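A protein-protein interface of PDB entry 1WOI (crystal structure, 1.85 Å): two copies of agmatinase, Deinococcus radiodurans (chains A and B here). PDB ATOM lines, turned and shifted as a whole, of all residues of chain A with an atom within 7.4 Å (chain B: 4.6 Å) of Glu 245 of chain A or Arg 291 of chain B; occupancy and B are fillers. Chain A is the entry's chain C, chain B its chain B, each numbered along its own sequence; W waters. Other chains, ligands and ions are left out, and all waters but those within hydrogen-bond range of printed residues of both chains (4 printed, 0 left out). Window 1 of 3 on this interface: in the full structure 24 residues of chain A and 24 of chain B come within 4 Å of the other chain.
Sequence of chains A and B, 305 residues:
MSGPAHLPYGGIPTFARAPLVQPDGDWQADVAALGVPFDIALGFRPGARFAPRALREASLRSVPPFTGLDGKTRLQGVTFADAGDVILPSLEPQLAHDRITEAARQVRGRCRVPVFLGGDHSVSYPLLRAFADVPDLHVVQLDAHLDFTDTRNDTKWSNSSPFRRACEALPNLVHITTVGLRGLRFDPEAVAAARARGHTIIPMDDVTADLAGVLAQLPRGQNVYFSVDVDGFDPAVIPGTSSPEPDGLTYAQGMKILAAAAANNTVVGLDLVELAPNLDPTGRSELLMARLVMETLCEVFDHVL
Glu 245 of chain A touches just one residue of chain B: Arg 291. Arg 291 of chain B touches four residues of chain A. Ala 290 of chain B touches none of the printed residues of chain A. Of the printed residues of chain B, Leu 184 of chain A touches Arg 291 and Glu 295. Of the printed residues of chain B, Pro 244 of chain A touches Leu 287 (3.8 Å). Of the printed residues of chain A, Ser 62 of chain B touches Arg 185. Met 294 of chain B touches none of the printed residues of chain A.
The guanidinium group (NH1) of Arg 291 of chain B lies within salt-bridge range of the side-chain carboxylate (OE2) of Glu 245 of chain A, 2.7 Å away.
Hydrophobic or aromatic side chains of chain B that line the printed part of chain A: Tyr 251, Leu 287 and Leu 288. Along chain B the printed residues that touch a printed residue of chain A span positions 62 to 295. Of the 23 printed residues of chain A, 7 touch a printed residue of chain B. Printed residues of chain A that touch a printed residue of chain B: Gly 183, Leu 184, Arg 185, Pro 244, Glu 245, Pro 246 and Asp 247.
No position is printed for both chains. Of the 10 pairs that touch across the chains among the printed residues, none has its exchanged pair printed and touching as well.
Arg 291 of chain B touches Gly 183 of chain A. Leu 184 of chain A touches Arg 291 of chain B (CD1 to CG, 3.8 Å). CD2 of Leu 184 of chain A touches CD of Glu 295 of chain B (3.8 Å). Ser 62 of chain B touches Arg 185 of chain A. Pro 244 of chain A touches Leu 287 of chain B (CG to CD1, 3.8 Å). CG of Tyr 251 of chain B touches CB of Pro 246 of chain A, at 3.5 Å. Leu 288 of chain B touches Pro 246 of chain A. NH1 of Arg 291 of chain B touches CG of Pro 246 of chain A (3.6 Å). OD2 of Asp 247 of chain A touches CD2 of Tyr 251 of chain B, 3.1 Å away.
OH of Tyr 251 of chain B lies within hydrogen-bond range of NE of Arg 291 of chain B. The backbone NH of Leu 292 of chain B lies close to the side-chain hydroxyl of Tyr 251 of chain B (3.3 Å). The side-chain hydroxyl (OH) of Tyr 251 of chain B sits at hydrogen-bond distance from the side-chain carboxylate (OE2) of Glu 295 of chain B (2.7 Å). NH2 of Arg 182 of chain A sits at hydrogen-bond distance from O of Glu 245 of chain A (2.9 Å). The guanidinium group (NE) of Arg 182 of chain A is in hydrogen-bond range of the backbone carbonyl oxygen (O) of Pro 246 of chain A, 3.0 Å away. The side-chain carboxylate (OD2) of Asp 234 of chain A lies close to the backbone NH (N) of Asp 247 of chain A (3.2 Å).
Water W4 lies within hydrogen-bond range of the backbone carbonyl oxygen of Pro 246 of chain A (2.8 Å) and the guanidinium group of Arg 291 of chain B (3.0 Å). Water W3 lies within hydrogen-bond range of the side-chain carboxylate (OD1) of Asp 247 of chain A (2.9 Å) and the backbone NH (N) of Tyr 251 of chain B (2.9 Å). Water W2 bridges the guanidinium group of Arg 291 of chain B (3.0 Å) and the backbone NH of Gly 183 of chain A (3.0 Å). Water W1 bridges the guanidinium group of Arg 185 of chain A (3.1 Å) and the backbone NH of Ser 62 of chain B (3.4 Å).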
ATOM      1  N   ALA A 144       7.350 -17.735 -25.821  1.00  0.00           N
ATOM      2  CA  ALA A 144       8.062 -17.234 -24.653  1.00  0.00           C
ATOM      3  C   ALA A 144       8.125 -15.710 -24.817  1.00  0.00           C
ATOM      4  O   ALA A 144       8.269 -14.973 -23.839  1.00  0.00           O
ATOM      5  CB  ALA A 144       9.469 -17.808 -24.602  1.00  0.00           C
ATOM      6  N   HIS A 145       8.017 -15.253 -26.061  1.00  0.00           N
ATOM      7  CA  HIS A 145       8.076 -13.824 -26.370  1.00  0.00           C
ATOM      8  C   HIS A 145       6.746 -13.294 -26.901  1.00  0.00           C
ATOM      9  O   HIS A 145       5.967 -14.027 -27.506  1.00  0.00           O
ATOM     10  CB  HIS A 145       9.168 -13.544 -27.406  1.00  0.00           C
ATOM     11  CG  HIS A 145      10.422 -14.334 -27.194  1.00  0.00           C
ATOM     12  ND1 HIS A 145      10.591 -15.608 -27.692  1.00  0.00           N
ATOM     13  CD2 HIS A 145      11.564 -14.035 -26.530  1.00  0.00           C
ATOM     14  CE1 HIS A 145      11.784 -16.059 -27.347  1.00  0.00           C
ATOM     15  NE2 HIS A 145      12.394 -15.124 -26.641  1.00  0.00           N
ATOM     16  N   GLY A 180       2.698 -18.343 -22.060  1.00  0.00           N
ATOM     17  CA  GLY A 180       4.057 -18.835 -21.903  1.00  0.00           C
ATOM     18  C   GLY A 180       5.136 -17.777 -21.804  1.00  0.00           C
ATOM     19  O   GLY A 180       6.311 -18.106 -21.663  1.00  0.00           O
ATOM     20  N   LEU A 181       4.745 -16.507 -21.872  1.00  0.00           N
ATOM     21  CA  LEU A 181       5.708 -15.417 -21.812  1.00  0.00           C
ATOM     22  C   LEU A 181       6.622 -15.502 -20.604  1.00  0.00           C
ATOM     23  O   LEU A 181       6.187 -15.824 -19.500  1.00  0.00           O
ATOM     24  CB  LEU A 181       4.979 -14.069 -21.825  1.00  0.00           C
ATOM     25  CG  LEU A 181       4.148 -13.812 -23.087  1.00  0.00           C
ATOM     26  CD1 LEU A 181       3.482 -12.456 -23.009  1.00  0.00           C
ATOM     27  CD2 LEU A 181       5.056 -13.869 -24.305  1.00  0.00           C
ATOM     28  N   ARG A 182       7.896 -15.208 -20.824  1.00  0.00           N
ATOM     29  CA  ARG A 182       8.887 -15.246 -19.763  1.00  0.00           C
ATOM     30  C   ARG A 182      10.183 -14.627 -20.268  1.00  0.00           C
ATOM     31  O   ARG A 182      10.353 -14.420 -21.470  1.00  0.00           O
ATOM     32  CB  ARG A 182       9.117 -16.693 -19.321  1.00  0.00           C
ATOM     33  CG  ARG A 182       9.573 -17.618 -20.441  1.00  0.00           C
ATOM     34  CD  ARG A 182       9.494 -19.074 -20.011  1.00  0.00           C
ATOM     35  NE  ARG A 182      10.151 -19.971 -20.957  1.00  0.00           N
ATOM     36  CZ  ARG A 182       9.572 -20.529 -22.017  1.00  0.00           C
ATOM     37  NH1 ARG A 182       8.297 -20.298 -22.298  1.00  0.00           N
ATOM     38  NH2 ARG A 182      10.284 -21.327 -22.806  1.00  0.00           N
ATOM     39  N   GLY A 183      11.095 -14.318 -19.353  1.00  0.00           N
ATOM     40  CA  GLY A 183      12.352 -13.716 -19.754  1.00  0.00           C
ATOM     41  C   GLY A 183      12.636 -12.443 -18.990  1.00  0.00           C
ATOM     42  O   GLY A 183      11.759 -11.913 -18.300  1.00  0.00           O
ATOM     43  N   LEU A 184      13.862 -11.948 -19.112  1.00  0.00           N
ATOM     44  CA  LEU A 184      14.272 -10.735 -18.417  1.00  0.00           C
ATOM     45  C   LEU A 184      13.904  -9.469 -19.175  1.00  0.00           C
ATOM     46  O   LEU A 184      13.526  -8.464 -18.572  1.00  0.00           O
ATOM     47  CB  LEU A 184      15.785 -10.740 -18.184  1.00  0.00           C
ATOM     48  CG  LEU A 184      16.379 -11.873 -17.348  1.00  0.00           C
ATOM     49  CD1 LEU A 184      17.874 -11.644 -17.190  1.00  0.00           C
ATOM     50  CD2 LEU A 184      15.700 -11.926 -15.992  1.00  0.00           C
ATOM     51  N   ARG A 185      14.002  -9.521 -20.500  1.00  0.00           N
ATOM     52  CA  ARG A 185      13.717  -8.345 -21.305  1.00  0.00           C
ATOM     53  C   ARG A 185      12.432  -8.391 -22.112  1.00  0.00           C
ATOM     54  O   ARG A 185      12.139  -9.370 -22.799  1.00  0.00           O
ATOM     55  CB  ARG A 185      14.879  -8.074 -22.262  1.00  0.00           C
ATOM     56  CG  ARG A 185      14.823  -6.700 -22.917  1.00  0.00           C
ATOM     57  CD  ARG A 185      15.730  -6.627 -24.135  1.00  0.00           C
ATOM     58  NE  ARG A 185      17.044  -7.216 -23.882  1.00  0.00           N
ATOM     59  CZ  ARG A 185      17.919  -6.759 -22.993  1.00  0.00           C
ATOM     60  NH1 ARG A 185      17.633  -5.693 -22.256  1.00  0.00           N
ATOM     61  NH2 ARG A 185      19.082  -7.376 -22.842  1.00  0.00           N
ATOM     62  N   PHE A 186      11.666  -7.313 -22.015  1.00  0.00           N
ATOM     63  CA  PHE A 186      10.430  -7.175 -22.766  1.00  0.00           C
ATOM     64  C   PHE A 186      10.365  -5.762 -23.319  1.00  0.00           C
ATOM     65  O   PHE A 186      10.750  -4.806 -22.647  1.00  0.00           O
ATOM     66  CB  PHE A 186       9.209  -7.440 -21.890  1.00  0.00           C
ATOM     67  CG  PHE A 186       8.954  -8.893 -21.637  1.00  0.00           C
ATOM     68  CD1 PHE A 186       9.636  -9.567 -20.631  1.00  0.00           C
ATOM     69  CD2 PHE A 186       8.052  -9.596 -22.429  1.00  0.00           C
ATOM     70  CE1 PHE A 186       9.423 -10.927 -20.414  1.00  0.00           C
ATOM     71  CE2 PHE A 186       7.831 -10.957 -22.221  1.00  0.00           C
ATOM     72  CZ  PHE A 186       8.519 -11.622 -21.210  1.00  0.00           C
ATOM     73  N   ASP A 231       9.548 -22.196 -29.058  1.00  0.00           N
ATOM     74  CA  ASP A 231      10.274 -21.740 -27.878  1.00  0.00           C
ATOM     75  C   ASP A 231       9.365 -21.454 -26.690  1.00  0.00           C
ATOM     76  O   ASP A 231       9.834 -21.092 -25.619  1.00  0.00           O
ATOM     77  CB  ASP A 231      11.208 -20.549 -28.174  1.00  0.00           C
ATOM     78  CG  ASP A 231      10.483 -19.247 -28.468  1.00  0.00           C
ATOM     79  OD1 ASP A 231       9.340 -19.031 -28.010  1.00  0.00           O
ATOM     80  OD2 ASP A 231      11.105 -18.406 -29.152  1.00  0.00           O
ATOM     81  N   GLY A 232       8.062 -21.653 -26.879  1.00  0.00           N
ATOM     82  CA  GLY A 232       7.129 -21.480 -25.778  1.00  0.00           C
ATOM     83  C   GLY A 232       7.347 -22.666 -24.848  1.00  0.00           C
ATOM     84  O   GLY A 232       7.108 -22.584 -23.640  1.00  0.00           O
ATOM     85  N   PHE A 233       7.818 -23.775 -25.418  1.00  0.00           N
ATOM     86  CA  PHE A 233       8.093 -24.992 -24.647  1.00  0.00           C
ATOM     87  C   PHE A 233       9.448 -24.888 -23.961  1.00  0.00           C
ATOM     88  O   PHE A 233      10.335 -24.172 -24.426  1.00  0.00           O
ATOM     89  CB  PHE A 233       8.067 -26.230 -25.554  1.00  0.00           C
ATOM     90  CG  PHE A 233       6.706 -26.536 -26.113  1.00  0.00           C
ATOM     91  CD1 PHE A 233       6.336 -26.086 -27.378  1.00  0.00           C
ATOM     92  CD2 PHE A 233       5.776 -27.231 -25.349  1.00  0.00           C
ATOM     93  CE1 PHE A 233       5.054 -26.323 -27.869  1.00  0.00           C
ATOM     94  CE2 PHE A 233       4.495 -27.470 -25.829  1.00  0.00           C
ATOM     95  CZ  PHE A 233       4.133 -27.015 -27.093  1.00  0.00           C
ATOM     96  N   ASP A 234       9.603 -25.592 -22.848  1.00  0.00           N
ATOM     97  CA  ASP A 234      10.862 -25.562 -22.106  1.00  0.00           C
ATOM     98  C   ASP A 234      12.003 -26.054 -22.987  1.00  0.00           C
ATOM     99  O   ASP A 234      11.857 -27.043 -23.702  1.00  0.00           O
ATOM    100  CB  ASP A 234      10.764 -26.444 -20.860  1.00  0.00           C
ATOM    101  CG  ASP A 234      11.881 -26.174 -19.866  1.00  0.00           C
ATOM    102  OD1 ASP A 234      13.005 -26.691 -20.046  1.00  0.00           O
ATOM    103  OD2 ASP A 234      11.629 -25.419 -18.903  1.00  0.00           O
ATOM    104  N   PRO A 235      13.154 -25.365 -22.942  1.00  0.00           N
ATOM    105  CA  PRO A 235      14.358 -25.685 -23.715  1.00  0.00           C
ATOM    106  C   PRO A 235      14.851 -27.108 -23.458  1.00  0.00           C
ATOM    107  O   PRO A 235      15.497 -27.709 -24.313  1.00  0.00           O
ATOM    108  CB  PRO A 235      15.367 -24.637 -23.243  1.00  0.00           C
ATOM    109  CG  PRO A 235      14.513 -23.501 -22.798  1.00  0.00           C
ATOM    110  CD  PRO A 235      13.367 -24.168 -22.108  1.00  0.00           C
ATOM    111  N   ALA A 236      14.564 -27.643 -22.272  1.00  0.00           N
ATOM    112  CA  ALA A 236      14.971 -29.010 -21.960  1.00  0.00           C
ATOM    113  C   ALA A 236      14.154 -29.970 -22.828  1.00  0.00           C
ATOM    114  O   ALA A 236      14.645 -31.014 -23.251  1.00  0.00           O
ATOM    115  CB  ALA A 236      14.733 -29.310 -20.490  1.00  0.00           C
ATOM    116  N   THR A 241      15.850 -24.416 -31.041  1.00  0.00           N
ATOM    117  CA  THR A 241      15.237 -23.131 -31.362  1.00  0.00           C
ATOM    118  C   THR A 241      16.257 -22.011 -31.142  1.00  0.00           C
ATOM    119  O   THR A 241      17.162 -22.124 -30.310  1.00  0.00           O
ATOM    120  CB  THR A 241      13.955 -22.904 -30.523  1.00  0.00           C
ATOM    121  OG1 THR A 241      13.192 -21.838 -31.099  1.00  0.00           O
ATOM    122  CG2 THR A 241      14.297 -22.546 -29.088  1.00  0.00           C
ATOM    123  N   SER A 243      16.192 -18.761 -29.810  1.00  0.00           N
ATOM    124  CA  SER A 243      16.297 -18.052 -28.541  1.00  0.00           C
ATOM    125  C   SER A 243      15.509 -18.692 -27.417  1.00  0.00           C
ATOM    126  O   SER A 243      14.405 -18.256 -27.098  1.00  0.00           O
ATOM    127  CB  SER A 243      15.816 -16.614 -28.736  1.00  0.00           C
ATOM    128  OG  SER A 243      16.389 -16.052 -29.901  1.00  0.00           O
ATOM    129  N   PRO A 244      16.072 -19.732 -26.794  1.00  0.00           N
ATOM    130  CA  PRO A 244      15.387 -20.416 -25.698  1.00  0.00           C
ATOM    131  C   PRO A 244      15.375 -19.613 -24.407  1.00  0.00           C
ATOM    132  O   PRO A 244      16.285 -18.815 -24.137  1.00  0.00           O
ATOM    133  CB  PRO A 244      16.166 -21.725 -25.570  1.00  0.00           C
ATOM    134  CG  PRO A 244      17.559 -21.309 -25.934  1.00  0.00           C
ATOM    135  CD  PRO A 244      17.336 -20.409 -27.135  1.00  0.00           C
ATOM    136  N   GLU A 245      14.329 -19.833 -23.624  1.00  0.00           N
ATOM    137  CA  GLU A 245      14.153 -19.168 -22.346  1.00  0.00           C
ATOM    138  C   GLU A 245      13.823 -20.277 -21.353  1.00  0.00           C
ATOM    139  O   GLU A 245      12.932 -21.091 -21.599  1.00  0.00           O
ATOM    140  CB  GLU A 245      13.001 -18.169 -22.439  1.00  0.00           C
ATOM    141  CG  GLU A 245      13.174 -16.962 -21.557  1.00  0.00           C
ATOM    142  CD  GLU A 245      14.441 -16.200 -21.876  1.00  0.00           C
ATOM    143  OE1 GLU A 245      14.557 -15.651 -22.991  1.00  0.00           O
ATOM    144  OE2 GLU A 245      15.329 -16.159 -21.007  1.00  0.00           O
ATOM    145  N   PRO A 246      14.548 -20.338 -20.227  1.00  0.00           N
ATOM    146  CA  PRO A 246      14.289 -21.382 -19.231  1.00  0.00           C
ATOM    147  C   PRO A 246      12.876 -21.380 -18.659  1.00  0.00           C
ATOM    148  O   PRO A 246      12.147 -20.396 -18.781  1.00  0.00           O
ATOM    149  CB  PRO A 246      15.340 -21.103 -18.157  1.00  0.00           C
ATOM    150  CG  PRO A 246      15.494 -19.606 -18.228  1.00  0.00           C
ATOM    151  CD  PRO A 246      15.549 -19.375 -19.732  1.00  0.00           C
ATOM    152  N   ASP A 247      12.512 -22.507 -18.049  1.00  0.00           N
ATOM    153  CA  ASP A 247      11.222 -22.702 -17.396  1.00  0.00           C
ATOM    154  C   ASP A 247       9.998 -22.440 -18.259  1.00  0.00           C
ATOM    155  O   ASP A 247       9.188 -21.551 -17.964  1.00  0.00           O
ATOM    156  CB  ASP A 247      11.161 -21.844 -16.126  1.00  0.00           C
ATOM    157  CG  ASP A 247      12.362 -22.063 -15.220  1.00  0.00           C
ATOM    158  OD1 ASP A 247      12.585 -23.213 -14.775  1.00  0.00           O
ATOM    159  OD2 ASP A 247      13.091 -21.086 -14.961  1.00  0.00           O
ATOM    160  N   GLY A 248       9.854 -23.237 -19.311  1.00  0.00           N
ATOM    161  CA  GLY A 248       8.722 -23.090 -20.201  1.00  0.00           C
ATOM    162  C   GLY A 248       7.704 -24.204 -20.075  1.00  0.00           C
ATOM    163  O   GLY A 248       7.702 -24.977 -19.110  1.00  0.00           O
ATOM    164  N   LEU A 249       6.831 -24.289 -21.071  1.00  0.00           N
ATOM    165  CA  LEU A 249       5.783 -25.297 -21.100  1.00  0.00           C
ATOM    166  C   LEU A 249       6.323 -26.698 -21.317  1.00  0.00           C
ATOM    167  O   LEU A 249       7.281 -26.888 -22.054  1.00  0.00           O
ATOM    168  CB  LEU A 249       4.808 -25.010 -22.244  1.00  0.00           C
ATOM    169  CG  LEU A 249       4.074 -23.679 -22.324  1.00  0.00           C
ATOM    170  CD1 LEU A 249       3.517 -23.513 -23.741  1.00  0.00           C
ATOM    171  CD2 LEU A 249       2.952 -23.644 -21.286  1.00  0.00           C
ATOM    172  N   SER B  62      21.714 -11.223 -23.104  1.00  0.00           N
ATOM    173  CA  SER B  62      21.226 -10.598 -21.877  1.00  0.00           C
ATOM    174  C   SER B  62      21.976  -9.322 -21.488  1.00  0.00           C
ATOM    175  O   SER B  62      22.542  -9.240 -20.396  1.00  0.00           O
ATOM    176  CB  SER B  62      21.314 -11.599 -20.721  1.00  0.00           C
ATOM    177  OG  SER B  62      20.640 -12.807 -21.037  1.00  0.00           O
ATOM    178  N   TYR B 251      15.830 -24.315 -13.417  1.00  0.00           N
ATOM    179  CA  TYR B 251      16.384 -22.973 -13.426  1.00  0.00           C
ATOM    180  C   TYR B 251      15.671 -22.124 -12.368  1.00  0.00           C
ATOM    181  O   TYR B 251      16.314 -21.413 -11.589  1.00  0.00           O
ATOM    182  CB  TYR B 251      16.187 -22.337 -14.804  1.00  0.00           C
ATOM    183  CG  TYR B 251      16.696 -20.917 -14.905  1.00  0.00           C
ATOM    184  CD1 TYR B 251      17.952 -20.640 -15.447  1.00  0.00           C
ATOM    185  CD2 TYR B 251      15.925 -19.846 -14.446  1.00  0.00           C
ATOM    186  CE1 TYR B 251      18.428 -19.329 -15.531  1.00  0.00           C
ATOM    187  CE2 TYR B 251      16.391 -18.541 -14.521  1.00  0.00           C
ATOM    188  CZ  TYR B 251      17.640 -18.288 -15.063  1.00  0.00           C
ATOM    189  OH  TYR B 251      18.103 -16.995 -15.132  1.00  0.00           O
ATOM    190  N   LEU B 287      23.609 -20.259 -22.625  1.00  0.00           N
ATOM    191  CA  LEU B 287      22.578 -19.224 -22.710  1.00  0.00           C
ATOM    192  C   LEU B 287      21.824 -19.067 -21.388  1.00  0.00           C
ATOM    193  O   LEU B 287      21.618 -17.951 -20.905  1.00  0.00           O
ATOM    194  CB  LEU B 287      21.583 -19.542 -23.831  1.00  0.00           C
ATOM    195  CG  LEU B 287      22.096 -19.369 -25.265  1.00  0.00           C
ATOM    196  CD1 LEU B 287      21.008 -19.751 -26.259  1.00  0.00           C
ATOM    197  CD2 LEU B 287      22.514 -17.921 -25.483  1.00  0.00           C
ATOM    198  N   LEU B 288      21.416 -20.189 -20.804  1.00  0.00           N
ATOM    199  CA  LEU B 288      20.677 -20.162 -19.552  1.00  0.00           C
ATOM    200  C   LEU B 288      21.538 -19.720 -18.377  1.00  0.00           C
ATOM    201  O   LEU B 288      21.069 -18.988 -17.505  1.00  0.00           O
ATOM    202  CB  LEU B 288      20.073 -21.544 -19.264  1.00  0.00           C
ATOM    203  CG  LEU B 288      18.635 -21.784 -19.741  1.00  0.00           C
ATOM    204  CD1 LEU B 288      18.501 -21.463 -21.223  1.00  0.00           C
ATOM    205  CD2 LEU B 288      18.258 -23.230 -19.461  1.00  0.00           C
ATOM    206  N   MET B 289      22.800 -20.145 -18.350  1.00  0.00           N
ATOM    207  CA  MET B 289      23.672 -19.767 -17.242  1.00  0.00           C
ATOM    208  C   MET B 289      24.117 -18.310 -17.306  1.00  0.00           C
ATOM    209  O   MET B 289      24.314 -17.679 -16.266  1.00  0.00           O
ATOM    210  CB  MET B 289      24.885 -20.699 -17.161  1.00  0.00           C
ATOM    211  CG  MET B 289      24.562 -22.133 -16.706  1.00  0.00           C
ATOM    212  SD  MET B 289      23.690 -22.269 -15.093  1.00  0.00           S
ATOM    213  CE  MET B 289      24.188 -20.799 -14.317  1.00  0.00           C
ATOM    214  N   ALA B 290      24.279 -17.767 -18.512  1.00  0.00           N
ATOM    215  CA  ALA B 290      24.653 -16.361 -18.634  1.00  0.00           C
ATOM    216  C   ALA B 290      23.466 -15.555 -18.105  1.00  0.00           C
ATOM    217  O   ALA B 290      23.640 -14.538 -17.429  1.00  0.00           O
ATOM    218  CB  ALA B 290      24.937 -16.000 -20.088  1.00  0.00           C
ATOM    219  N   ARG B 291      22.255 -16.018 -18.407  1.00  0.00           N
ATOM    220  CA  ARG B 291      21.060 -15.335 -17.932  1.00  0.00           C
ATOM    221  C   ARG B 291      20.962 -15.424 -16.411  1.00  0.00           C
ATOM    222  O   ARG B 291      20.538 -14.472 -15.755  1.00  0.00           O
ATOM    223  CB  ARG B 291      19.781 -15.937 -18.532  1.00  0.00           C
ATOM    224  CG  ARG B 291      18.542 -15.302 -17.922  1.00  0.00           C
ATOM    225  CD  ARG B 291      17.237 -15.993 -18.255  1.00  0.00           C
ATOM    226  NE  ARG B 291      16.267 -15.727 -17.194  1.00  0.00           N
ATOM    227  CZ  ARG B 291      14.950 -15.818 -17.332  1.00  0.00           C
ATOM    228  NH1 ARG B 291      14.419 -16.164 -18.496  1.00  0.00           N
ATOM    229  NH2 ARG B 291      14.160 -15.575 -16.294  1.00  0.00           N
ATOM    230  N   LEU B 292      21.344 -16.570 -15.852  1.00  0.00           N
ATOM    231  CA  LEU B 292      21.278 -16.754 -14.407  1.00  0.00           C
ATOM    232  C   LEU B 292      22.128 -15.704 -13.706  1.00  0.00           C
ATOM    233  O   LEU B 292      21.712 -15.129 -12.695  1.00  0.00           O
ATOM    234  CB  LEU B 292      21.781 -18.146 -14.002  1.00  0.00           C
ATOM    235  CG  LEU B 292      21.560 -18.475 -12.517  1.00  0.00           C
ATOM    236  CD1 LEU B 292      20.143 -19.009 -12.342  1.00  0.00           C
ATOM    237  CD2 LEU B 292      22.563 -19.513 -12.030  1.00  0.00           C
ATOM    238  N   VAL B 293      23.325 -15.475 -14.237  1.00  0.00           N
ATOM    239  CA  VAL B 293      24.239 -14.494 -13.664  1.00  0.00           C
ATOM    240  C   VAL B 293      23.627 -13.096 -13.740  1.00  0.00           C
ATOM    241  O   VAL B 293      23.632 -12.356 -12.758  1.00  0.00           O
ATOM    242  CB  VAL B 293      25.609 -14.507 -14.395  1.00  0.00           C
ATOM    243  CG1 VAL B 293      26.498 -13.384 -13.880  1.00  0.00           C
ATOM    244  CG2 VAL B 293      26.302 -15.843 -14.174  1.00  0.00           C
ATOM    245  N   MET B 294      23.081 -12.742 -14.900  1.00  0.00           N
ATOM    246  CA  MET B 294      22.477 -11.424 -15.064  1.00  0.00           C
ATOM    247  C   MET B 294      21.250 -11.251 -14.175  1.00  0.00           C
ATOM    248  O   MET B 294      21.039 -10.184 -13.588  1.00  0.00           O
ATOM    249  CB  MET B 294      22.097 -11.185 -16.528  1.00  0.00           C
ATOM    250  CG  MET B 294      23.285 -11.104 -17.481  1.00  0.00           C
ATOM    251  SD  MET B 294      24.573  -9.937 -16.968  1.00  0.00           S
ATOM    252  CE  MET B 294      23.623  -8.428 -16.828  1.00  0.00           C
ATOM    253  N   GLU B 295      20.436 -12.296 -14.070  1.00  0.00           N
ATOM    254  CA  GLU B 295      19.241 -12.223 -13.239  1.00  0.00           C
ATOM    255  C   GLU B 295      19.616 -12.132 -11.761  1.00  0.00           C
ATOM    256  O   GLU B 295      18.945 -11.462 -10.978  1.00  0.00           O
ATOM    257  CB  GLU B 295      18.343 -13.440 -13.481  1.00  0.00           C
ATOM    258  CG  GLU B 295      17.062 -13.404 -12.672  1.00  0.00           C
ATOM    259  CD  GLU B 295      16.050 -14.436 -13.126  1.00  0.00           C
ATOM    260  OE1 GLU B 295      14.955 -14.489 -12.529  1.00  0.00           O
ATOM    261  OE2 GLU B 295      16.347 -15.192 -14.079  1.00  0.00           O
HETATM  262  O   HOH W   1      20.880  -8.543 -25.034  1.00  0.00           O
HETATM  263  O   HOH W   2      11.204 -15.160 -16.458  1.00  0.00           O
HETATM  264  O   HOH W   3      14.344 -25.245 -15.745  1.00  0.00           O
HETATM  265  O   HOH W   4      12.032 -17.779 -17.770  1.00  0.00           O
